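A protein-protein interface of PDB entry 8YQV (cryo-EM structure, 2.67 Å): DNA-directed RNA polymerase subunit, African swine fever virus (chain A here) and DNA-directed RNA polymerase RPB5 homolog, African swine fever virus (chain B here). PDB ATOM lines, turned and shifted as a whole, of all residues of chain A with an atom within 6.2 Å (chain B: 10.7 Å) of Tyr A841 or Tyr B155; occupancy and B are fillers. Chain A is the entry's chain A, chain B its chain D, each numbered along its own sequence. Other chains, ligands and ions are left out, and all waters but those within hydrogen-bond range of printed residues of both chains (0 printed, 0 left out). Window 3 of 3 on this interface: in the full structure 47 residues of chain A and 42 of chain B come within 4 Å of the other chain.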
ATOM      1  N   VAL A 838     -26.182 -17.820  -4.218  1.00  0.00           N
ATOM      2  CA  VAL A 838     -27.372 -16.975  -4.223  1.00  0.00           C
ATOM      3  C   VAL A 838     -27.253 -15.917  -3.133  1.00  0.00           C
ATOM      4  O   VAL A 838     -26.928 -16.225  -1.983  1.00  0.00           O
ATOM      5  CB  VAL A 838     -28.641 -17.823  -4.050  1.00  0.00           C
ATOM      6  CG1 VAL A 838     -29.865 -16.948  -4.047  1.00  0.00           C
ATOM      7  CG2 VAL A 838     -28.740 -18.829  -5.152  1.00  0.00           C
ATOM      8  N   ASP A 839     -27.520 -14.664  -3.502  1.00  0.00           N
ATOM      9  CA  ASP A 839     -27.466 -13.520  -2.600  1.00  0.00           C
ATOM     10  C   ASP A 839     -28.733 -13.438  -1.765  1.00  0.00           C
ATOM     11  O   ASP A 839     -29.582 -14.329  -1.781  1.00  0.00           O
ATOM     12  CB  ASP A 839     -27.315 -12.224  -3.383  1.00  0.00           C
ATOM     13  CG  ASP A 839     -26.019 -12.123  -4.091  1.00  0.00           C
ATOM     14  OD1 ASP A 839     -25.200 -13.053  -3.970  1.00  0.00           O
ATOM     15  OD2 ASP A 839     -25.816 -11.102  -4.773  1.00  0.00           O
ATOM     16  N   TYR A 840     -28.889 -12.333  -1.045  1.00  0.00           N
ATOM     17  CA  TYR A 840     -30.143 -12.006  -0.389  1.00  0.00           C
ATOM     18  C   TYR A 840     -31.148 -11.380  -1.336  1.00  0.00           C
ATOM     19  O   TYR A 840     -32.296 -11.156  -0.944  1.00  0.00           O
ATOM     20  CB  TYR A 840     -29.894 -11.074   0.793  1.00  0.00           C
ATOM     21  CG  TYR A 840     -29.201 -11.757   1.936  1.00  0.00           C
ATOM     22  CD1 TYR A 840     -29.778 -12.838   2.565  1.00  0.00           C
ATOM     23  CD2 TYR A 840     -27.968 -11.329   2.381  1.00  0.00           C
ATOM     24  CE1 TYR A 840     -29.150 -13.474   3.590  1.00  0.00           C
ATOM     25  CE2 TYR A 840     -27.337 -11.957   3.410  1.00  0.00           C
ATOM     26  CZ  TYR A 840     -27.933 -13.028   4.015  1.00  0.00           C
ATOM     27  OH  TYR A 840     -27.306 -13.664   5.052  1.00  0.00           O
ATOM     28  N   TYR A 841     -30.744 -11.092  -2.565  1.00  0.00           N
ATOM     29  CA  TYR A 841     -31.639 -10.604  -3.596  1.00  0.00           C
ATOM     30  C   TYR A 841     -32.052 -11.697  -4.563  1.00  0.00           C
ATOM     31  O   TYR A 841     -32.679 -11.397  -5.579  1.00  0.00           O
ATOM     32  CB  TYR A 841     -30.977  -9.463  -4.358  1.00  0.00           C
ATOM     33  CG  TYR A 841     -30.808  -8.199  -3.568  1.00  0.00           C
ATOM     34  CD1 TYR A 841     -29.743  -8.038  -2.706  1.00  0.00           C
ATOM     35  CD2 TYR A 841     -31.697  -7.155  -3.705  1.00  0.00           C
ATOM     36  CE1 TYR A 841     -29.584  -6.884  -1.989  1.00  0.00           C
ATOM     37  CE2 TYR A 841     -31.542  -5.998  -2.993  1.00  0.00           C
ATOM     38  CZ  TYR A 841     -30.485  -5.866  -2.142  1.00  0.00           C
ATOM     39  OH  TYR A 841     -30.340  -4.705  -1.433  1.00  0.00           O
ATOM     40  N   ARG A 842     -31.715 -12.951  -4.268  1.00  0.00           N
ATOM     41  CA  ARG A 842     -31.861 -14.091  -5.171  1.00  0.00           C
ATOM     42  C   ARG A 842     -31.007 -13.945  -6.419  1.00  0.00           C
ATOM     43  O   ARG A 842     -31.181 -14.693  -7.381  1.00  0.00           O
ATOM     44  CB  ARG A 842     -33.321 -14.335  -5.569  1.00  0.00           C
ATOM     45  CG  ARG A 842     -34.041 -15.399  -4.772  1.00  0.00           C
ATOM     46  CD  ARG A 842     -34.287 -14.921  -3.389  1.00  0.00           C
ATOM     47  NE  ARG A 842     -35.096 -15.835  -2.599  1.00  0.00           N
ATOM     48  CZ  ARG A 842     -36.247 -15.512  -2.030  1.00  0.00           C
ATOM     49  NH1 ARG A 842     -36.798 -14.328  -2.213  1.00  0.00           N
ATOM     50  NH2 ARG A 842     -36.844 -16.389  -1.236  1.00  0.00           N
ATOM     51  N   ARG A 843     -30.089 -12.988  -6.423  1.00  0.00           N
ATOM     52  CA  ARG A 843     -29.107 -12.878  -7.483  1.00  0.00           C
ATOM     53  C   ARG A 843     -28.049 -13.955  -7.319  1.00  0.00           C
ATOM     54  O   ARG A 843     -27.891 -14.551  -6.256  1.00  0.00           O
ATOM     55  CB  ARG A 843     -28.430 -11.513  -7.462  1.00  0.00           C
ATOM     56  CG  ARG A 843     -29.358 -10.332  -7.442  1.00  0.00           C
ATOM     57  CD  ARG A 843     -28.562  -9.077  -7.614  1.00  0.00           C
ATOM     58  NE  ARG A 843     -27.574  -8.936  -6.555  1.00  0.00           N
ATOM     59  CZ  ARG A 843     -27.568  -7.963  -5.658  1.00  0.00           C
ATOM     60  NH1 ARG A 843     -28.447  -6.983  -5.699  1.00  0.00           N
ATOM     61  NH2 ARG A 843     -26.648  -7.970  -4.702  1.00  0.00           N
ATOM     62  N   GLN A 853     -28.879 -11.732 -12.600  1.00  0.00           N
ATOM     63  CA  GLN A 853     -29.697 -10.776 -11.865  1.00  0.00           C
ATOM     64  C   GLN A 853     -30.732 -11.476 -10.998  1.00  0.00           C
ATOM     65  O   GLN A 853     -31.081 -10.978  -9.927  1.00  0.00           O
ATOM     66  CB  GLN A 853     -30.377  -9.818 -12.837  1.00  0.00           C
ATOM     67  CG  GLN A 853     -31.148  -8.712 -12.176  1.00  0.00           C
ATOM     68  CD  GLN A 853     -30.255  -7.733 -11.471  1.00  0.00           C
ATOM     69  OE1 GLN A 853     -29.260  -7.284 -12.030  1.00  0.00           O
ATOM     70  NE2 GLN A 853     -30.597  -7.392 -10.242  1.00  0.00           N
ATOM     71  N   LEU A 854     -31.247 -12.611 -11.449  1.00  0.00           N
ATOM     72  CA  LEU A 854     -32.118 -13.458 -10.655  1.00  0.00           C
ATOM     73  C   LEU A 854     -31.763 -14.891 -10.993  1.00  0.00           C
ATOM     74  O   LEU A 854     -31.520 -15.203 -12.155  1.00  0.00           O
ATOM     75  CB  LEU A 854     -33.593 -13.183 -10.944  1.00  0.00           C
ATOM     76  CG  LEU A 854     -34.635 -13.720  -9.967  1.00  0.00           C
ATOM     77  CD1 LEU A 854     -34.564 -13.020  -8.637  1.00  0.00           C
ATOM     78  CD2 LEU A 854     -35.993 -13.537 -10.559  1.00  0.00           C
ATOM     79  N   PHE A 975     -41.143 -11.930  -4.211  1.00  0.00           N
ATOM     80  CA  PHE A 975     -39.698 -11.839  -4.279  1.00  0.00           C
ATOM     81  C   PHE A 975     -39.108 -10.844  -3.296  1.00  0.00           C
ATOM     82  O   PHE A 975     -37.882 -10.781  -3.185  1.00  0.00           O
ATOM     83  CB  PHE A 975     -39.268 -11.465  -5.693  1.00  0.00           C
ATOM     84  CG  PHE A 975     -39.615 -12.491  -6.712  1.00  0.00           C
ATOM     85  CD1 PHE A 975     -38.933 -13.686  -6.765  1.00  0.00           C
ATOM     86  CD2 PHE A 975     -40.625 -12.266  -7.619  1.00  0.00           C
ATOM     87  CE1 PHE A 975     -39.253 -14.630  -7.697  1.00  0.00           C
ATOM     88  CE2 PHE A 975     -40.944 -13.207  -8.550  1.00  0.00           C
ATOM     89  CZ  PHE A 975     -40.256 -14.388  -8.591  1.00  0.00           C
ATOM     90  N   TYR A 990     -36.952  -6.108 -13.060  1.00  0.00           N
ATOM     91  CA  TYR A 990     -36.592  -7.507 -13.242  1.00  0.00           C
ATOM     92  C   TYR A 990     -37.414  -8.426 -12.348  1.00  0.00           C
ATOM     93  O   TYR A 990     -37.506  -9.625 -12.620  1.00  0.00           O
ATOM     94  CB  TYR A 990     -35.098  -7.705 -13.002  1.00  0.00           C
ATOM     95  CG  TYR A 990     -34.665  -7.674 -11.558  1.00  0.00           C
ATOM     96  CD1 TYR A 990     -34.499  -6.475 -10.889  1.00  0.00           C
ATOM     97  CD2 TYR A 990     -34.401  -8.846 -10.871  1.00  0.00           C
ATOM     98  CE1 TYR A 990     -34.100  -6.446  -9.584  1.00  0.00           C
ATOM     99  CE2 TYR A 990     -34.002  -8.823  -9.569  1.00  0.00           C
ATOM    100  CZ  TYR A 990     -33.851  -7.621  -8.929  1.00  0.00           C
ATOM    101  OH  TYR A 990     -33.448  -7.597  -7.621  1.00  0.00           O
ATOM    102  N   LEU A 991     -38.014  -7.897 -11.281  1.00  0.00           N
ATOM    103  CA  LEU A 991     -38.928  -8.698 -10.476  1.00  0.00           C
ATOM    104  C   LEU A 991     -40.334  -8.702 -11.052  1.00  0.00           C
ATOM    105  O   LEU A 991     -41.094  -9.641 -10.808  1.00  0.00           O
ATOM    106  CB  LEU A 991     -38.965  -8.198  -9.034  1.00  0.00           C
ATOM    107  CG  LEU A 991     -37.703  -8.397  -8.206  1.00  0.00           C
ATOM    108  CD1 LEU A 991     -37.944  -7.954  -6.793  1.00  0.00           C
ATOM    109  CD2 LEU A 991     -37.254  -9.835  -8.250  1.00  0.00           C
ATOM    110  N   TYR A1037     -31.443 -18.314   0.054  1.00  0.00           N
ATOM    111  CA  TYR A1037     -30.275 -17.459   0.194  1.00  0.00           C
ATOM    112  C   TYR A1037     -29.064 -18.307   0.531  1.00  0.00           C
ATOM    113  O   TYR A1037     -29.121 -19.146   1.432  1.00  0.00           O
ATOM    114  CB  TYR A1037     -30.502 -16.439   1.301  1.00  0.00           C
ATOM    115  CG  TYR A1037     -31.678 -15.525   1.112  1.00  0.00           C
ATOM    116  CD1 TYR A1037     -32.033 -15.059  -0.134  1.00  0.00           C
ATOM    117  CD2 TYR A1037     -32.440 -15.132   2.193  1.00  0.00           C
ATOM    118  CE1 TYR A1037     -33.098 -14.217  -0.289  1.00  0.00           C
ATOM    119  CE2 TYR A1037     -33.509 -14.299   2.041  1.00  0.00           C
ATOM    120  CZ  TYR A1037     -33.837 -13.847   0.801  1.00  0.00           C
ATOM    121  OH  TYR A1037     -34.909 -13.007   0.650  1.00  0.00           O
ATOM    122  N   ALA B 147     -30.073   4.350 -13.510  1.00  0.00           N
ATOM    123  CA  ALA B 147     -29.071   3.383 -13.085  1.00  0.00           C
ATOM    124  C   ALA B 147     -28.637   3.629 -11.649  1.00  0.00           C
ATOM    125  O   ALA B 147     -28.422   2.678 -10.894  1.00  0.00           O
ATOM    126  CB  ALA B 147     -27.867   3.432 -14.013  1.00  0.00           C
ATOM    127  N   GLN B 148     -28.486   4.893 -11.254  1.00  0.00           N
ATOM    128  CA  GLN B 148     -28.086   5.173  -9.882  1.00  0.00           C
ATOM    129  C   GLN B 148     -29.146   4.728  -8.893  1.00  0.00           C
ATOM    130  O   GLN B 148     -28.808   4.174  -7.845  1.00  0.00           O
ATOM    131  CB  GLN B 148     -27.777   6.657  -9.688  1.00  0.00           C
ATOM    132  CG  GLN B 148     -26.463   7.107 -10.308  1.00  0.00           C
ATOM    133  CD  GLN B 148     -25.298   6.209  -9.952  1.00  0.00           C
ATOM    134  OE1 GLN B 148     -25.134   5.809  -8.802  1.00  0.00           O
ATOM    135  NE2 GLN B 148     -24.484   5.880 -10.948  1.00  0.00           N
ATOM    136  N   GLU B 149     -30.426   4.946  -9.197  1.00  0.00           N
ATOM    137  CA  GLU B 149     -31.451   4.489  -8.264  1.00  0.00           C
ATOM    138  C   GLU B 149     -31.546   2.966  -8.242  1.00  0.00           C
ATOM    139  O   GLU B 149     -31.763   2.379  -7.175  1.00  0.00           O
ATOM    140  CB  GLU B 149     -32.802   5.130  -8.584  1.00  0.00           C
ATOM    141  CG  GLU B 149     -33.560   4.537  -9.741  1.00  0.00           C
ATOM    142  CD  GLU B 149     -34.795   5.342 -10.091  1.00  0.00           C
ATOM    143  OE1 GLU B 149     -34.976   6.433  -9.512  1.00  0.00           O
ATOM    144  OE2 GLU B 149     -35.587   4.886 -10.942  1.00  0.00           O
ATOM    145  N   PHE B 150     -31.348   2.310  -9.388  1.00  0.00           N
ATOM    146  CA  PHE B 150     -31.316   0.851  -9.414  1.00  0.00           C
ATOM    147  C   PHE B 150     -30.190   0.315  -8.543  1.00  0.00           C
ATOM    148  O   PHE B 150     -30.394  -0.588  -7.723  1.00  0.00           O
ATOM    149  CB  PHE B 150     -31.160   0.368 -10.858  1.00  0.00           C
ATOM    150  CG  PHE B 150     -30.831  -1.092 -10.983  1.00  0.00           C
ATOM    151  CD1 PHE B 150     -31.809  -2.051 -10.831  1.00  0.00           C
ATOM    152  CD2 PHE B 150     -29.543  -1.500 -11.261  1.00  0.00           C
ATOM    153  CE1 PHE B 150     -31.506  -3.382 -10.947  1.00  0.00           C
ATOM    154  CE2 PHE B 150     -29.240  -2.830 -11.374  1.00  0.00           C
ATOM    155  CZ  PHE B 150     -30.222  -3.771 -11.219  1.00  0.00           C
ATOM    156  N   LEU B 151     -28.992   0.879  -8.694  1.00  0.00           N
ATOM    157  CA  LEU B 151     -27.841   0.418  -7.930  1.00  0.00           C
ATOM    158  C   LEU B 151     -27.981   0.741  -6.452  1.00  0.00           C
ATOM    159  O   LEU B 151     -27.531  -0.035  -5.606  1.00  0.00           O
ATOM    160  CB  LEU B 151     -26.564   1.037  -8.490  1.00  0.00           C
ATOM    161  CG  LEU B 151     -26.156   0.663  -9.913  1.00  0.00           C
ATOM    162  CD1 LEU B 151     -25.129   1.641 -10.419  1.00  0.00           C
ATOM    163  CD2 LEU B 151     -25.613  -0.738  -9.971  1.00  0.00           C
ATOM    164  N   GLY B 152     -28.586   1.880  -6.119  1.00  0.00           N
ATOM    165  CA  GLY B 152     -28.823   2.198  -4.727  1.00  0.00           C
ATOM    166  C   GLY B 152     -29.810   1.263  -4.067  1.00  0.00           C
ATOM    167  O   GLY B 152     -29.633   0.891  -2.904  1.00  0.00           O
ATOM    168  N   ARG B 153     -30.864   0.876  -4.784  1.00  0.00           N
ATOM    169  CA  ARG B 153     -31.773  -0.132  -4.252  1.00  0.00           C
ATOM    170  C   ARG B 153     -31.076  -1.479  -4.110  1.00  0.00           C
ATOM    171  O   ARG B 153     -31.334  -2.218  -3.156  1.00  0.00           O
ATOM    172  CB  ARG B 153     -33.005  -0.247  -5.145  1.00  0.00           C
ATOM    173  CG  ARG B 153     -34.147  -1.044  -4.555  1.00  0.00           C
ATOM    174  CD  ARG B 153     -34.226  -2.435  -5.142  1.00  0.00           C
ATOM    175  NE  ARG B 153     -35.270  -3.221  -4.500  1.00  0.00           N
ATOM    176  CZ  ARG B 153     -35.353  -4.541  -4.549  1.00  0.00           C
ATOM    177  NH1 ARG B 153     -34.474  -5.262  -5.220  1.00  0.00           N
ATOM    178  NH2 ARG B 153     -36.341  -5.152  -3.906  1.00  0.00           N
ATOM    179  N   GLU B 154     -30.189  -1.809  -5.040  1.00  0.00           N
ATOM    180  CA  GLU B 154     -29.524  -3.102  -5.044  1.00  0.00           C
ATOM    181  C   GLU B 154     -28.244  -3.136  -4.221  1.00  0.00           C
ATOM    182  O   GLU B 154     -27.655  -4.211  -4.083  1.00  0.00           O
ATOM    183  CB  GLU B 154     -29.210  -3.516  -6.482  1.00  0.00           C
ATOM    184  CG  GLU B 154     -30.436  -3.752  -7.331  1.00  0.00           C
ATOM    185  CD  GLU B 154     -31.033  -5.113  -7.120  1.00  0.00           C
ATOM    186  OE1 GLU B 154     -30.269  -6.095  -7.092  1.00  0.00           O
ATOM    187  OE2 GLU B 154     -32.265  -5.207  -6.973  1.00  0.00           O
ATOM    188  N   TYR B 155     -27.805  -2.004  -3.673  1.00  0.00           N
ATOM    189  CA  TYR B 155     -26.543  -1.908  -2.939  1.00  0.00           C
ATOM    190  C   TYR B 155     -25.379  -2.414  -3.782  1.00  0.00           C
ATOM    191  O   TYR B 155     -24.532  -3.177  -3.324  1.00  0.00           O
ATOM    192  CB  TYR B 155     -26.609  -2.658  -1.608  1.00  0.00           C
ATOM    193  CG  TYR B 155     -27.330  -1.920  -0.514  1.00  0.00           C
ATOM    194  CD1 TYR B 155     -26.706  -0.913   0.197  1.00  0.00           C
ATOM    195  CD2 TYR B 155     -28.634  -2.238  -0.189  1.00  0.00           C
ATOM    196  CE1 TYR B 155     -27.366  -0.241   1.193  1.00  0.00           C
ATOM    197  CE2 TYR B 155     -29.299  -1.572   0.803  1.00  0.00           C
ATOM    198  CZ  TYR B 155     -28.663  -0.576   1.493  1.00  0.00           C
ATOM    199  OH  TYR B 155     -29.331   0.086   2.488  1.00  0.00           O
ATOM    200  N   LEU B 156     -25.344  -1.976  -5.033  1.00  0.00           N
ATOM    201  CA  LEU B 156     -24.346  -2.421  -5.988  1.00  0.00           C
ATOM    202  C   LEU B 156     -23.495  -1.246  -6.442  1.00  0.00           C
ATOM    203  O   LEU B 156     -23.950  -0.101  -6.474  1.00  0.00           O
ATOM    204  CB  LEU B 156     -24.994  -3.074  -7.209  1.00  0.00           C
ATOM    205  CG  LEU B 156     -25.594  -4.469  -7.090  1.00  0.00           C
ATOM    206  CD1 LEU B 156     -26.342  -4.808  -8.347  1.00  0.00           C
ATOM    207  CD2 LEU B 156     -24.523  -5.493  -6.834  1.00  0.00           C
ATOM    208  N   GLN B 157     -22.264  -1.539  -6.769  1.00  0.00           N
ATOM    209  CA  GLN B 157     -21.401  -0.628  -7.490  1.00  0.00           C
ATOM    210  C   GLN B 157     -21.422  -0.975  -8.967  1.00  0.00           C
ATOM    211  O   GLN B 157     -21.671  -2.124  -9.338  1.00  0.00           O
ATOM    212  CB  GLN B 157     -19.967  -0.711  -6.957  1.00  0.00           C
ATOM    213  CG  GLN B 157     -19.838  -0.497  -5.464  1.00  0.00           C
ATOM    214  CD  GLN B 157     -20.348   0.856  -5.023  1.00  0.00           C
ATOM    215  OE1 GLN B 157     -20.142   1.862  -5.698  1.00  0.00           O
ATOM    216  NE2 GLN B 157     -21.021   0.888  -3.883  1.00  0.00           N
ATOM    217  N   PRO B 158     -21.169  -0.007  -9.851  1.00  0.00           N
ATOM    218  CA  PRO B 158     -21.207  -0.304 -11.289  1.00  0.00           C
ATOM    219  C   PRO B 158     -20.248  -1.396 -11.715  1.00  0.00           C
ATOM    220  O   PRO B 158     -20.459  -1.996 -12.773  1.00  0.00           O
ATOM    221  CB  PRO B 158     -20.842   1.038 -11.930  1.00  0.00           C
ATOM    222  CG  PRO B 158     -21.263   2.040 -10.937  1.00  0.00           C
ATOM    223  CD  PRO B 158     -20.989   1.430  -9.599  1.00  0.00           C
ATOM    224  N   GLN B 159     -19.211  -1.674 -10.935  1.00  0.00           N
ATOM    225  CA  GLN B 159     -18.277  -2.747 -11.238  1.00  0.00           C
ATOM    226  C   GLN B 159     -18.802  -4.120 -10.852  1.00  0.00           C
ATOM    227  O   GLN B 159     -18.223  -5.126 -11.271  1.00  0.00           O
ATOM    228  CB  GLN B 159     -16.951  -2.499 -10.525  1.00  0.00           C
ATOM    229  CG  GLN B 159     -16.068  -1.475 -11.197  1.00  0.00           C
ATOM    230  CD  GLN B 159     -16.610  -0.069 -11.081  1.00  0.00           C
ATOM    231  OE1 GLN B 159     -16.753   0.637 -12.077  1.00  0.00           O
ATOM    232  NE2 GLN B 159     -16.925   0.343  -9.861  1.00  0.00           N
ATOM    233  N   ASP B 160     -19.872  -4.188 -10.063  1.00  0.00           N
ATOM    234  CA  ASP B 160     -20.465  -5.462  -9.689  1.00  0.00           C
ATOM    235  C   ASP B 160     -21.389  -6.024 -10.757  1.00  0.00           C
ATOM    236  O   ASP B 160     -21.717  -7.210 -10.698  1.00  0.00           O
ATOM    237  CB  ASP B 160     -21.240  -5.317  -8.381  1.00  0.00           C
ATOM    238  CG  ASP B 160     -20.376  -4.826  -7.240  1.00  0.00           C
ATOM    239  OD1 ASP B 160     -19.191  -5.209  -7.177  1.00  0.00           O
ATOM    240  OD2 ASP B 160     -20.884  -4.073  -6.388  1.00  0.00           O
ATOM    241  N   LEU B 161     -21.804  -5.218 -11.726  1.00  0.00           N
ATOM    242  CA  LEU B 161     -22.698  -5.669 -12.775  1.00  0.00           C
ATOM    243  C   LEU B 161     -21.950  -6.520 -13.793  1.00  0.00           C
ATOM    244  O   LEU B 161     -20.723  -6.501 -13.872  1.00  0.00           O
ATOM    245  CB  LEU B 161     -23.335  -4.480 -13.485  1.00  0.00           C
ATOM    246  CG  LEU B 161     -24.212  -3.529 -12.689  1.00  0.00           C
ATOM    247  CD1 LEU B 161     -24.674  -2.411 -13.588  1.00  0.00           C
ATOM    248  CD2 LEU B 161     -25.391  -4.261 -12.100  1.00  0.00           C
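The side-chain carboxylate (OE2) of Glu B154 is in hydrogen-bond range of the side-chain hydroxyl (OH) of Tyr A990, 2.7 Å away.
The side-chain hydroxyl (OH) of Tyr A841 sits at hydrogen-bond distance from the backbone carbonyl oxygen (O) of Arg B153, at 3.2 Å.
NE2 of Gln A853 lies within hydrogen-bond range of OE1 of Glu B154 (3.4 Å).
The side-chain carboxylate of Glu B154 is in salt-bridge range of the guanidinium group of Arg A843.
The side-chain carboxylate (OD2) of Asp A839 lies within salt-bridge range of the guanidinium group (NH2) of Arg A843 (3.2 Å).
The backbone carbonyl oxygen (O) of Leu B151 lies within hydrogen-bond range of the backbone NH (N) of Leu B156, 3.0 Å away.
The guanidinium group of Arg B153 lies within salt-bridge range of the side-chain carboxylate of Glu B154 (2.8 Å).
O of Glu B154 touches OH of Tyr A841, 3.8 Å away.
CD2 of Tyr B155 touches OH of Tyr A841, at 3.2 Å.
Leu B156 touches Arg A843 (CD2 to NH2, 3.9 Å).
Phe B150 touches Gln A853.
Tyr A990 touches Arg B153 (OH to NH1, 3.5 Å).
Tyr A841 touches just these residues of chain B: Arg B153, Glu B154 and Tyr B155.
Tyr B155 touches one residue of chain A.
No residue of chain B comes within 4 Å of Asp A839.
Of the printed residues of chain A, Phe B150 touches Gln A853.
Of the printed residues of chain A, Leu B156 touches Arg A843 (3.9 Å).
Of the printed residues of chain A, Arg B153 touches Tyr A841 and Tyr A990.
Printed residues of chain A within 4 Å of Glu B154: Tyr A841 (3.8 Å), Arg A843 (2.5 Å), Gln A853 (3.4 Å) and Tyr A990 (2.7 Å).
Of the printed residues of chain B, Tyr A990 touches Arg B153 (3.5 Å) and Glu B154 (2.7 Å).
Leu A854 touches none of the printed residues of chain B.
The nearest residue of chain B that does not touch Tyr A841 is Gly B152 (5.8 Å).
The nearest residue of chain A that does not touch Tyr B155 is Arg A843 (5.4 Å).
The nearest printed residue of chain A that does not touch Leu B156 is Gln A853 (5.3 Å).
Hydrophobic or aromatic side chains of chain A that line the printed part of chain B: Tyr A841 and Tyr A990.
Of the 15 printed residues of chain B, 5 touch a printed residue of chain A.
Printed residues of chain B that touch a printed residue of chain A: Phe B150, Arg B153, Glu B154, Tyr B155 and Leu B156.
Hydrophobic or aromatic side chains of chain B within 4 Å of the printed part of chain A: Phe B150, Tyr B155 and Leu B156.
Among the printed residues, Asp or Glu carboxylates within 4 Å of a Lys or Arg side-chain nitrogen of the other chain: Arg A843 with Glu B154 (2.5 Å).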
